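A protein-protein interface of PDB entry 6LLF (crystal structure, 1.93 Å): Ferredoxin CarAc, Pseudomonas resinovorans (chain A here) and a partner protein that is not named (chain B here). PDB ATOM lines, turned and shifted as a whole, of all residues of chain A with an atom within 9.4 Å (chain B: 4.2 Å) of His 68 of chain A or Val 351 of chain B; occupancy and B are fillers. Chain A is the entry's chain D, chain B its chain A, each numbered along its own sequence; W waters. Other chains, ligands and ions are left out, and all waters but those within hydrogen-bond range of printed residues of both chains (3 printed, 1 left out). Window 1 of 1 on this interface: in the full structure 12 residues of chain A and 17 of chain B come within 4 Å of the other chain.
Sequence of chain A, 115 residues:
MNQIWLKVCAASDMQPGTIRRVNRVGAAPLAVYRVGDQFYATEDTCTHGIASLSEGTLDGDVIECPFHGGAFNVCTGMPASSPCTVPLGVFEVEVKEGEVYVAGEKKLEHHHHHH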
ATOM      1  N   CYS A  46       8.644  -5.371   3.241  1.00  0.00           N
ATOM      2  CA  CYS A  46       9.047  -6.211   2.082  1.00  0.00           C
ATOM      3  C   CYS A  46      10.455  -5.775   1.624  1.00  0.00           C
ATOM      4  O   CYS A  46      10.682  -4.558   1.540  1.00  0.00           O
ATOM      5  CB  CYS A  46       8.043  -6.063   0.946  1.00  0.00           C
ATOM      6  SG  CYS A  46       8.415  -7.161  -0.437  1.00  0.00           S
ATOM      7  N   THR A  47      11.361  -6.719   1.377  1.00  0.00           N
ATOM      8  CA  THR A  47      12.771  -6.453   0.971  1.00  0.00           C
ATOM      9  C   THR A  47      12.808  -5.861  -0.444  1.00  0.00           C
ATOM     10  O   THR A  47      13.838  -5.281  -0.835  1.00  0.00           O
ATOM     11  CB  THR A  47      13.662  -7.703   0.987  1.00  0.00           C
ATOM     12  OG1 THR A  47      13.202  -8.712   0.081  1.00  0.00           O
ATOM     13  CG2 THR A  47      13.768  -8.342   2.352  1.00  0.00           C
ATOM     14  N   HIS A  48      11.732  -6.009  -1.203  1.00  0.00           N
ATOM     15  CA  HIS A  48      11.666  -5.479  -2.588  1.00  0.00           C
ATOM     16  C   HIS A  48      11.262  -4.002  -2.600  1.00  0.00           C
ATOM     17  O   HIS A  48      11.199  -3.445  -3.682  1.00  0.00           O
ATOM     18  CB  HIS A  48      10.723  -6.347  -3.434  1.00  0.00           C
ATOM     19  CG  HIS A  48      10.576  -5.891  -4.850  1.00  0.00           C
ATOM     20  ND1 HIS A  48       9.445  -5.250  -5.298  1.00  0.00           N
ATOM     21  CD2 HIS A  48      11.396  -6.020  -5.926  1.00  0.00           C
ATOM     22  CE1 HIS A  48       9.558  -5.035  -6.605  1.00  0.00           C
ATOM     23  NE2 HIS A  48      10.760  -5.482  -7.017  1.00  0.00           N
ATOM     24  N   GLY A  49      10.924  -3.393  -1.467  1.00  0.00           N
ATOM     25  CA  GLY A  49      10.369  -2.030  -1.493  1.00  0.00           C
ATOM     26  C   GLY A  49      10.103  -1.474  -0.113  1.00  0.00           C
ATOM     27  O   GLY A  49      11.030  -1.510   0.738  1.00  0.00           O
ATOM     28  N   ILE A  50       8.924  -0.888   0.053  1.00  0.00           N
ATOM     29  CA  ILE A  50       8.494  -0.234   1.318  1.00  0.00           C
ATOM     30  C   ILE A  50       7.106  -0.724   1.746  1.00  0.00           C
ATOM     31  O   ILE A  50       6.521  -0.089   2.645  1.00  0.00           O
ATOM     32  CB  ILE A  50       8.535   1.291   1.154  1.00  0.00           C
ATOM     33  CG1 ILE A  50       7.640   1.790   0.021  1.00  0.00           C
ATOM     34  CG2 ILE A  50       9.982   1.740   0.986  1.00  0.00           C
ATOM     35  CD1 ILE A  50       7.473   3.308  -0.023  1.00  0.00           C
ATOM     36  N   ALA A  51       6.606  -1.821   1.173  1.00  0.00           N
ATOM     37  CA  ALA A  51       5.312  -2.424   1.576  1.00  0.00           C
ATOM     38  C   ALA A  51       5.390  -3.020   2.996  1.00  0.00           C
ATOM     39  O   ALA A  51       6.451  -3.558   3.407  1.00  0.00           O
ATOM     40  CB  ALA A  51       4.955  -3.500   0.572  1.00  0.00           C
ATOM     41  N   SER A  52       4.270  -2.979   3.701  1.00  0.00           N
ATOM     42  CA  SER A  52       4.017  -3.703   4.971  1.00  0.00           C
ATOM     43  C   SER A  52       3.424  -5.085   4.660  1.00  0.00           C
ATOM     44  O   SER A  52       2.287  -5.151   4.178  1.00  0.00           O
ATOM     45  CB  SER A  52       3.100  -2.881   5.840  1.00  0.00           C
ATOM     46  OG  SER A  52       2.612  -3.675   6.902  1.00  0.00           O
ATOM     47  N   LEU A  53       4.182  -6.158   4.892  1.00  0.00           N
ATOM     48  CA  LEU A  53       3.774  -7.566   4.621  1.00  0.00           C
ATOM     49  C   LEU A  53       2.549  -7.926   5.481  1.00  0.00           C
ATOM     50  O   LEU A  53       1.767  -8.831   5.060  1.00  0.00           O
ATOM     51  CB  LEU A  53       4.930  -8.524   4.928  1.00  0.00           C
ATOM     52  CG  LEU A  53       6.105  -8.477   3.961  1.00  0.00           C
ATOM     53  CD1 LEU A  53       7.245  -9.377   4.445  1.00  0.00           C
ATOM     54  CD2 LEU A  53       5.657  -8.882   2.555  1.00  0.00           C
ATOM     55  N   GLY A  56      -0.516  -7.945   3.663  1.00  0.00           N
ATOM     56  CA  GLY A  56      -0.516  -8.906   2.551  1.00  0.00           C
ATOM     57  C   GLY A  56      -1.520 -10.026   2.767  1.00  0.00           C
ATOM     58  O   GLY A  56      -2.482  -9.890   3.572  1.00  0.00           O
ATOM     59  N   GLU A  64       2.348 -13.127   0.784  1.00  0.00           N
ATOM     60  CA  GLU A  64       2.328 -12.386  -0.497  1.00  0.00           C
ATOM     61  C   GLU A  64       2.268 -10.889  -0.178  1.00  0.00           C
ATOM     62  O   GLU A  64       1.377 -10.470   0.607  1.00  0.00           O
ATOM     63  CB  GLU A  64       1.140 -12.819  -1.346  1.00  0.00           C
ATOM     64  CG  GLU A  64       1.042 -12.017  -2.619  1.00  0.00           C
ATOM     65  CD  GLU A  64      -0.269 -12.187  -3.372  1.00  0.00           C
ATOM     66  OE1 GLU A  64      -0.227 -12.884  -4.367  1.00  0.00           O
ATOM     67  OE2 GLU A  64      -1.304 -11.620  -2.936  1.00  0.00           O
ATOM     68  N   CYS A  65       3.172 -10.126  -0.783  1.00  0.00           N
ATOM     69  CA  CYS A  65       3.302  -8.666  -0.609  1.00  0.00           C
ATOM     70  C   CYS A  65       2.172  -7.969  -1.362  1.00  0.00           C
ATOM     71  O   CYS A  65       1.899  -8.315  -2.508  1.00  0.00           O
ATOM     72  CB  CYS A  65       4.659  -8.188  -1.128  1.00  0.00           C
ATOM     73  SG  CYS A  65       4.817  -6.390  -0.990  1.00  0.00           S
ATOM     74  N   PRO A  66       1.490  -6.970  -0.745  1.00  0.00           N
ATOM     75  CA  PRO A  66       0.358  -6.292  -1.379  1.00  0.00           C
ATOM     76  C   PRO A  66       0.759  -5.338  -2.523  1.00  0.00           C
ATOM     77  O   PRO A  66      -0.063  -5.080  -3.413  1.00  0.00           O
ATOM     78  CB  PRO A  66      -0.277  -5.539  -0.194  1.00  0.00           C
ATOM     79  CG  PRO A  66       0.868  -5.240   0.708  1.00  0.00           C
ATOM     80  CD  PRO A  66       1.760  -6.457   0.605  1.00  0.00           C
ATOM     81  N   PHE A  67       2.032  -4.896  -2.554  1.00  0.00           N
ATOM     82  CA  PHE A  67       2.536  -3.972  -3.608  1.00  0.00           C
ATOM     83  C   PHE A  67       2.611  -4.686  -4.953  1.00  0.00           C
ATOM     84  O   PHE A  67       1.970  -4.150  -5.879  1.00  0.00           O
ATOM     85  CB  PHE A  67       3.890  -3.380  -3.230  1.00  0.00           C
ATOM     86  CG  PHE A  67       3.823  -2.152  -2.367  1.00  0.00           C
ATOM     87  CD1 PHE A  67       2.713  -1.884  -1.574  1.00  0.00           C
ATOM     88  CD2 PHE A  67       4.894  -1.279  -2.322  1.00  0.00           C
ATOM     89  CE1 PHE A  67       2.678  -0.760  -0.748  1.00  0.00           C
ATOM     90  CE2 PHE A  67       4.852  -0.154  -1.511  1.00  0.00           C
ATOM     91  CZ  PHE A  67       3.748   0.101  -0.723  1.00  0.00           C
ATOM     92  N   HIS A  68       3.409  -5.758  -5.095  1.00  0.00           N
ATOM     93  CA  HIS A  68       3.772  -6.301  -6.431  1.00  0.00           C
ATOM     94  C   HIS A  68       3.530  -7.803  -6.520  1.00  0.00           C
ATOM     95  O   HIS A  68       3.759  -8.346  -7.597  1.00  0.00           O
ATOM     96  CB  HIS A  68       5.228  -5.948  -6.753  1.00  0.00           C
ATOM     97  CG  HIS A  68       5.535  -4.489  -6.637  1.00  0.00           C
ATOM     98  ND1 HIS A  68       6.460  -4.000  -5.748  1.00  0.00           N
ATOM     99  CD2 HIS A  68       5.029  -3.410  -7.293  1.00  0.00           C
ATOM    100  CE1 HIS A  68       6.546  -2.686  -5.866  1.00  0.00           C
ATOM    101  NE2 HIS A  68       5.680  -2.295  -6.812  1.00  0.00           N
ATOM    102  N   GLY A  69       3.027  -8.448  -5.454  1.00  0.00           N
ATOM    103  CA  GLY A  69       2.741  -9.899  -5.481  1.00  0.00           C
ATOM    104  C   GLY A  69       4.002 -10.733  -5.331  1.00  0.00           C
ATOM    105  O   GLY A  69       3.911 -11.952  -5.473  1.00  0.00           O
ATOM    106  N   GLY A  70       5.136 -10.119  -4.971  1.00  0.00           N
ATOM    107  CA  GLY A  70       6.283 -10.872  -4.445  1.00  0.00           C
ATOM    108  C   GLY A  70       5.873 -11.619  -3.185  1.00  0.00           C
ATOM    109  O   GLY A  70       4.834 -11.253  -2.559  1.00  0.00           O
ATOM    110  N   ALA A  71       6.608 -12.661  -2.830  1.00  0.00           N
ATOM    111  CA  ALA A  71       6.215 -13.552  -1.722  1.00  0.00           C
ATOM    112  C   ALA A  71       7.455 -14.140  -1.049  1.00  0.00           C
ATOM    113  O   ALA A  71       8.516 -14.247  -1.679  1.00  0.00           O
ATOM    114  CB  ALA A  71       5.274 -14.641  -2.215  1.00  0.00           C
ATOM    115  N   SER A  81       8.035 -15.953  -4.445  1.00  0.00           N
ATOM    116  CA  SER A  81       7.623 -15.400  -5.767  1.00  0.00           C
ATOM    117  C   SER A  81       8.422 -14.150  -6.145  1.00  0.00           C
ATOM    118  O   SER A  81       8.777 -13.345  -5.258  1.00  0.00           O
ATOM    119  CB  SER A  81       6.132 -15.113  -5.823  1.00  0.00           C
ATOM    120  OG  SER A  81       5.376 -16.251  -5.396  1.00  0.00           O
ATOM    121  N   SER A  82       8.664 -14.008  -7.441  1.00  0.00           N
ATOM    122  CA  SER A  82       9.150 -12.776  -8.112  1.00  0.00           C
ATOM    123  C   SER A  82       8.167 -11.659  -7.771  1.00  0.00           C
ATOM    124  O   SER A  82       6.994 -11.964  -7.482  1.00  0.00           O
ATOM    125  CB  SER A  82       9.267 -13.006  -9.590  1.00  0.00           C
ATOM    126  OG  SER A  82       7.988 -13.270 -10.162  1.00  0.00           O
ATOM    127  N   PRO A  83       8.589 -10.362  -7.741  1.00  0.00           N
ATOM    128  CA  PRO A  83       9.967  -9.931  -8.044  1.00  0.00           C
ATOM    129  C   PRO A  83      10.980  -9.992  -6.886  1.00  0.00           C
ATOM    130  O   PRO A  83      12.096  -9.521  -7.066  1.00  0.00           O
ATOM    131  CB  PRO A  83       9.774  -8.442  -8.402  1.00  0.00           C
ATOM    132  CG  PRO A  83       8.628  -8.000  -7.472  1.00  0.00           C
ATOM    133  CD  PRO A  83       7.697  -9.209  -7.457  1.00  0.00           C
ATOM    134  N   CYS A  84      10.599 -10.559  -5.733  1.00  0.00           N
ATOM    135  CA  CYS A  84      11.425 -10.574  -4.491  1.00  0.00           C
ATOM    136  C   CYS A  84      12.656 -11.462  -4.676  1.00  0.00           C
ATOM    137  O   CYS A  84      12.514 -12.559  -5.299  1.00  0.00           O
ATOM    138  CB  CYS A  84      10.629 -11.087  -3.311  1.00  0.00           C
ATOM    139  SG  CYS A  84       9.349  -9.904  -2.862  1.00  0.00           S
ATOM    140  N   ILE B   8      -0.909  -8.938 -14.319  1.00  0.00           N
ATOM    141  CA  ILE B   8      -0.211  -7.775 -13.698  1.00  0.00           C
ATOM    142  C   ILE B   8      -1.177  -7.093 -12.738  1.00  0.00           C
ATOM    143  O   ILE B   8      -0.763  -6.804 -11.598  1.00  0.00           O
ATOM    144  CB  ILE B   8       0.344  -6.815 -14.759  1.00  0.00           C
ATOM    145  CG1 ILE B   8       1.396  -7.530 -15.611  1.00  0.00           C
ATOM    146  CG2 ILE B   8       0.892  -5.560 -14.097  1.00  0.00           C
ATOM    147  CD1 ILE B   8       1.782  -6.794 -16.862  1.00  0.00           C
ATOM    148  N   ARG B  11      -1.396  -8.674  -9.413  1.00  0.00           N
ATOM    149  CA  ARG B  11      -0.216  -8.470  -8.533  1.00  0.00           C
ATOM    150  C   ARG B  11      -0.252  -7.121  -7.799  1.00  0.00           C
ATOM    151  O   ARG B  11       0.362  -7.033  -6.733  1.00  0.00           O
ATOM    152  CB  ARG B  11       1.079  -8.563  -9.337  1.00  0.00           C
ATOM    153  CG  ARG B  11       1.512  -9.991  -9.604  1.00  0.00           C
ATOM    154  CD  ARG B  11       2.673 -10.046 -10.582  1.00  0.00           C
ATOM    155  NE  ARG B  11       3.365 -11.329 -10.555  1.00  0.00           N
ATOM    156  CZ  ARG B  11       4.265 -11.697  -9.639  1.00  0.00           C
ATOM    157  NH1 ARG B  11       4.581 -10.872  -8.652  1.00  0.00           N
ATOM    158  NH2 ARG B  11       4.825 -12.909  -9.708  1.00  0.00           N
ATOM    159  N   LYS B 348       5.461  -3.892 -17.086  1.00  0.00           N
ATOM    160  CA  LYS B 348       6.158  -4.737 -16.083  1.00  0.00           C
ATOM    161  C   LYS B 348       6.881  -3.841 -15.051  1.00  0.00           C
ATOM    162  O   LYS B 348       7.168  -4.338 -13.972  1.00  0.00           O
ATOM    163  CB  LYS B 348       7.126  -5.733 -16.724  1.00  0.00           C
ATOM    164  CG  LYS B 348       6.521  -6.731 -17.718  1.00  0.00           C
ATOM    165  CD  LYS B 348       5.629  -7.744 -17.090  1.00  0.00           C
ATOM    166  CE  LYS B 348       4.961  -8.698 -18.075  1.00  0.00           C
ATOM    167  NZ  LYS B 348       5.893  -9.705 -18.638  1.00  0.00           N
ATOM    168  N   GLY B 349       7.173  -2.573 -15.341  1.00  0.00           N
ATOM    169  CA  GLY B 349       7.810  -1.686 -14.324  1.00  0.00           C
ATOM    170  C   GLY B 349       6.938  -1.554 -13.084  1.00  0.00           C
ATOM    171  O   GLY B 349       7.461  -1.267 -12.004  1.00  0.00           O
ATOM    172  N   TRP B 350       5.611  -1.720 -13.235  1.00  0.00           N
ATOM    173  CA  TRP B 350       4.611  -1.598 -12.145  1.00  0.00           C
ATOM    174  C   TRP B 350       4.771  -2.773 -11.172  1.00  0.00           C
ATOM    175  O   TRP B 350       4.265  -2.685 -10.050  1.00  0.00           O
ATOM    176  CB  TRP B 350       3.191  -1.508 -12.700  1.00  0.00           C
ATOM    177  CG  TRP B 350       2.945  -0.337 -13.588  1.00  0.00           C
ATOM    178  CD1 TRP B 350       2.654  -0.399 -14.913  1.00  0.00           C
ATOM    179  CD2 TRP B 350       2.900   1.056 -13.240  1.00  0.00           C
ATOM    180  NE1 TRP B 350       2.440   0.850 -15.419  1.00  0.00           N
ATOM    181  CE2 TRP B 350       2.557   1.762 -14.416  1.00  0.00           C
ATOM    182  CE3 TRP B 350       3.104   1.787 -12.058  1.00  0.00           C
ATOM    183  CZ2 TRP B 350       2.486   3.148 -14.468  1.00  0.00           C
ATOM    184  CZ3 TRP B 350       3.018   3.159 -12.101  1.00  0.00           C
ATOM    185  CH2 TRP B 350       2.707   3.826 -13.286  1.00  0.00           C
ATOM    186  N   VAL B 351       5.504  -3.811 -11.574  1.00  0.00           N
ATOM    187  CA  VAL B 351       5.820  -4.964 -10.694  1.00  0.00           C
ATOM    188  C   VAL B 351       7.274  -4.908 -10.230  1.00  0.00           C
ATOM    189  O   VAL B 351       7.532  -5.257  -9.080  1.00  0.00           O
ATOM    190  CB  VAL B 351       5.531  -6.258 -11.469  1.00  0.00           C
ATOM    191  CG1 VAL B 351       5.981  -7.463 -10.672  1.00  0.00           C
ATOM    192  CG2 VAL B 351       4.049  -6.361 -11.822  1.00  0.00           C
ATOM    193  N   ASN B 352       8.190  -4.537 -11.128  1.00  0.00           N
ATOM    194  CA  ASN B 352       9.644  -4.776 -10.979  1.00  0.00           C
ATOM    195  C   ASN B 352      10.346  -3.574 -10.327  1.00  0.00           C
ATOM    196  O   ASN B 352      11.476  -3.787  -9.869  1.00  0.00           O
ATOM    197  CB  ASN B 352      10.267  -5.165 -12.308  1.00  0.00           C
ATOM    198  CG  ASN B 352       9.859  -6.546 -12.766  1.00  0.00           C
ATOM    199  OD1 ASN B 352       9.842  -7.465 -11.958  1.00  0.00           O
ATOM    200  ND2 ASN B 352       9.541  -6.700 -14.047  1.00  0.00           N
ATOM    201  N   GLU B 353       9.751  -2.366 -10.330  1.00  0.00           N
ATOM    202  CA  GLU B 353      10.299  -1.194  -9.592  1.00  0.00           C
ATOM    203  C   GLU B 353      10.750  -1.619  -8.181  1.00  0.00           C
ATOM    204  O   GLU B 353      10.005  -2.321  -7.489  1.00  0.00           O
ATOM    205  CB  GLU B 353       9.246  -0.075  -9.572  1.00  0.00           C
ATOM    206  CG  GLU B 353       7.976  -0.417  -8.793  1.00  0.00           C
ATOM    207  CD  GLU B 353       6.809   0.545  -8.879  1.00  0.00           C
ATOM    208  OE1 GLU B 353       6.883   1.510  -9.659  1.00  0.00           O
ATOM    209  OE2 GLU B 353       5.802   0.315  -8.147  1.00  0.00           O
HETATM  210  O   HOH W   1      12.522  -6.189  -9.101  1.00  0.00           O
HETATM  211  O   HOH W   2       9.350  -1.850  -4.840  1.00  0.00           O
HETATM  212  O   HOH W   3       7.044 -10.977 -10.998  1.00  0.00           O
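Among the printed residues, merely in contact across the chains: His 68 of chain A with Trp 350 of chain B (3.0 Å), His 48 of chain A with Val 351 of chain B (3.2 Å), His 68 of chain A with Val 351 of chain B (3.2 Å), Pro 83 of chain A with Val 351 of chain B (3.4 Å), Pro 83 of chain A with Asn 352 of chain B (3.7 Å), Pro 83 of chain A with Arg 11 of chain B (3.7 Å), Gly 70 of chain A with Arg 11 of chain B (3.8 Å) and Pro 66 of chain A with Arg 11 of chain B (3.9 Å).
O of Glu 353 of chain B sits close to NE2 of His 48 of chain A (3.3 Å).
O of Asn 352 of chain B sits at hydrogen-bond distance from NE2 of His 48 of chain A, at 3.4 Å.
O of Arg 11 of chain B lies close to O of Phe 67 of chain A (3.4 Å).
O of Ser 82 of chain A is in hydrogen-bond range of NH1 of Arg 11 of chain B.
The backbone carbonyl oxygen (O) of Arg 11 of chain B lies within hydrogen-bond range of the backbone NH (N) of Gly 69 of chain A.
The backbone carbonyl oxygen (O) of His 68 of chain A is in hydrogen-bond range of the guanidinium group (NH1) of Arg 11 of chain B.
The side-chain carboxylate (OE2) of Glu 353 of chain B is in hydrogen-bond range of a ring nitrogen (NE2) of His 68 of chain A (2.9 Å).
Water W3 lies within hydrogen-bond range of OG of Ser 82 of chain A (2.6 Å) and NH2 of Arg 11 of chain B (3.2 Å).
Water W2 bridges the backbone carbonyl oxygen of His 48 of chain A and the backbone carbonyl oxygen of Glu 353 of chain B.
Water W1 lies within hydrogen-bond range of the backbone carbonyl oxygen of Asn 352 of chain B and a ring nitrogen (NE2) of His 48 of chain A.
O of Lys 348 of chain B sits at hydrogen-bond distance from ND2 of Asn 352 of chain B (3.3 Å).
The backbone NH (N) of Phe 67 of chain A sits close to the side-chain sulfur (SG) of Cys 65 of chain A.
SG of Cys 46 of chain A lies close to N of His 48 of chain A (3.6 Å).
N of Cys 65 of chain A lies within hydrogen-bond range of O of Gly 70 of chain A (2.7 Å).
Printed residues of chain B within 4 Å of Pro 66 of chain A: Arg 11.
Of chain B, only Arg 11, Trp 350, Val 351 and Glu 353 come within 4 Å of His 68 of chain A.
Of the printed residues of chain B, Gly 69 of chain A touches Arg 11 (3.3 Å).
Of the printed residues of chain B, Pro 83 of chain A touches Arg 11 (3.7 Å), Val 351 (3.4 Å) and Asn 352 (3.7 Å).
No residue of chain A comes within 4 Å of Gly 349 of chain B.
Of the printed residues of chain A, Trp 350 of chain B touches His 68 (3.0 Å).
Val 351 of chain B touches just these residues of chain A: His 48 (3.2 Å), His 68 (3.2 Å) and Pro 83 (3.4 Å).
Asn 352 of chain B touches just these residues of chain A: His 48 (3.4 Å) and Pro 83 (3.7 Å).
Glu 353 of chain B touches just these residues of chain A: His 48 (2.9 Å) and His 68 (2.9 Å).
The nearest residue of chain A that does not touch Val 351 of chain B is Ser 82 of chain A (5.5 Å).
The nearest printed residue of chain A that does not touch Arg 11 of chain B is Ser 81 of chain A (4.7 Å).
Printed residues of chain B that touch a printed residue of chain A: Arg 11, Trp 350, Val 351, Asn 352 and Glu 353.
Hydrophobic or aromatic side chains of chain B that line the printed part of chain A: Val 351.
Hydrophobic or aromatic side chains of chain A that line the printed part of chain B: His 48, His 68 and Pro 83.
Among the printed residues, no Asp or Glu carboxylate lies within 4 Å of a Lys or Arg side-chain nitrogen of the other chain.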
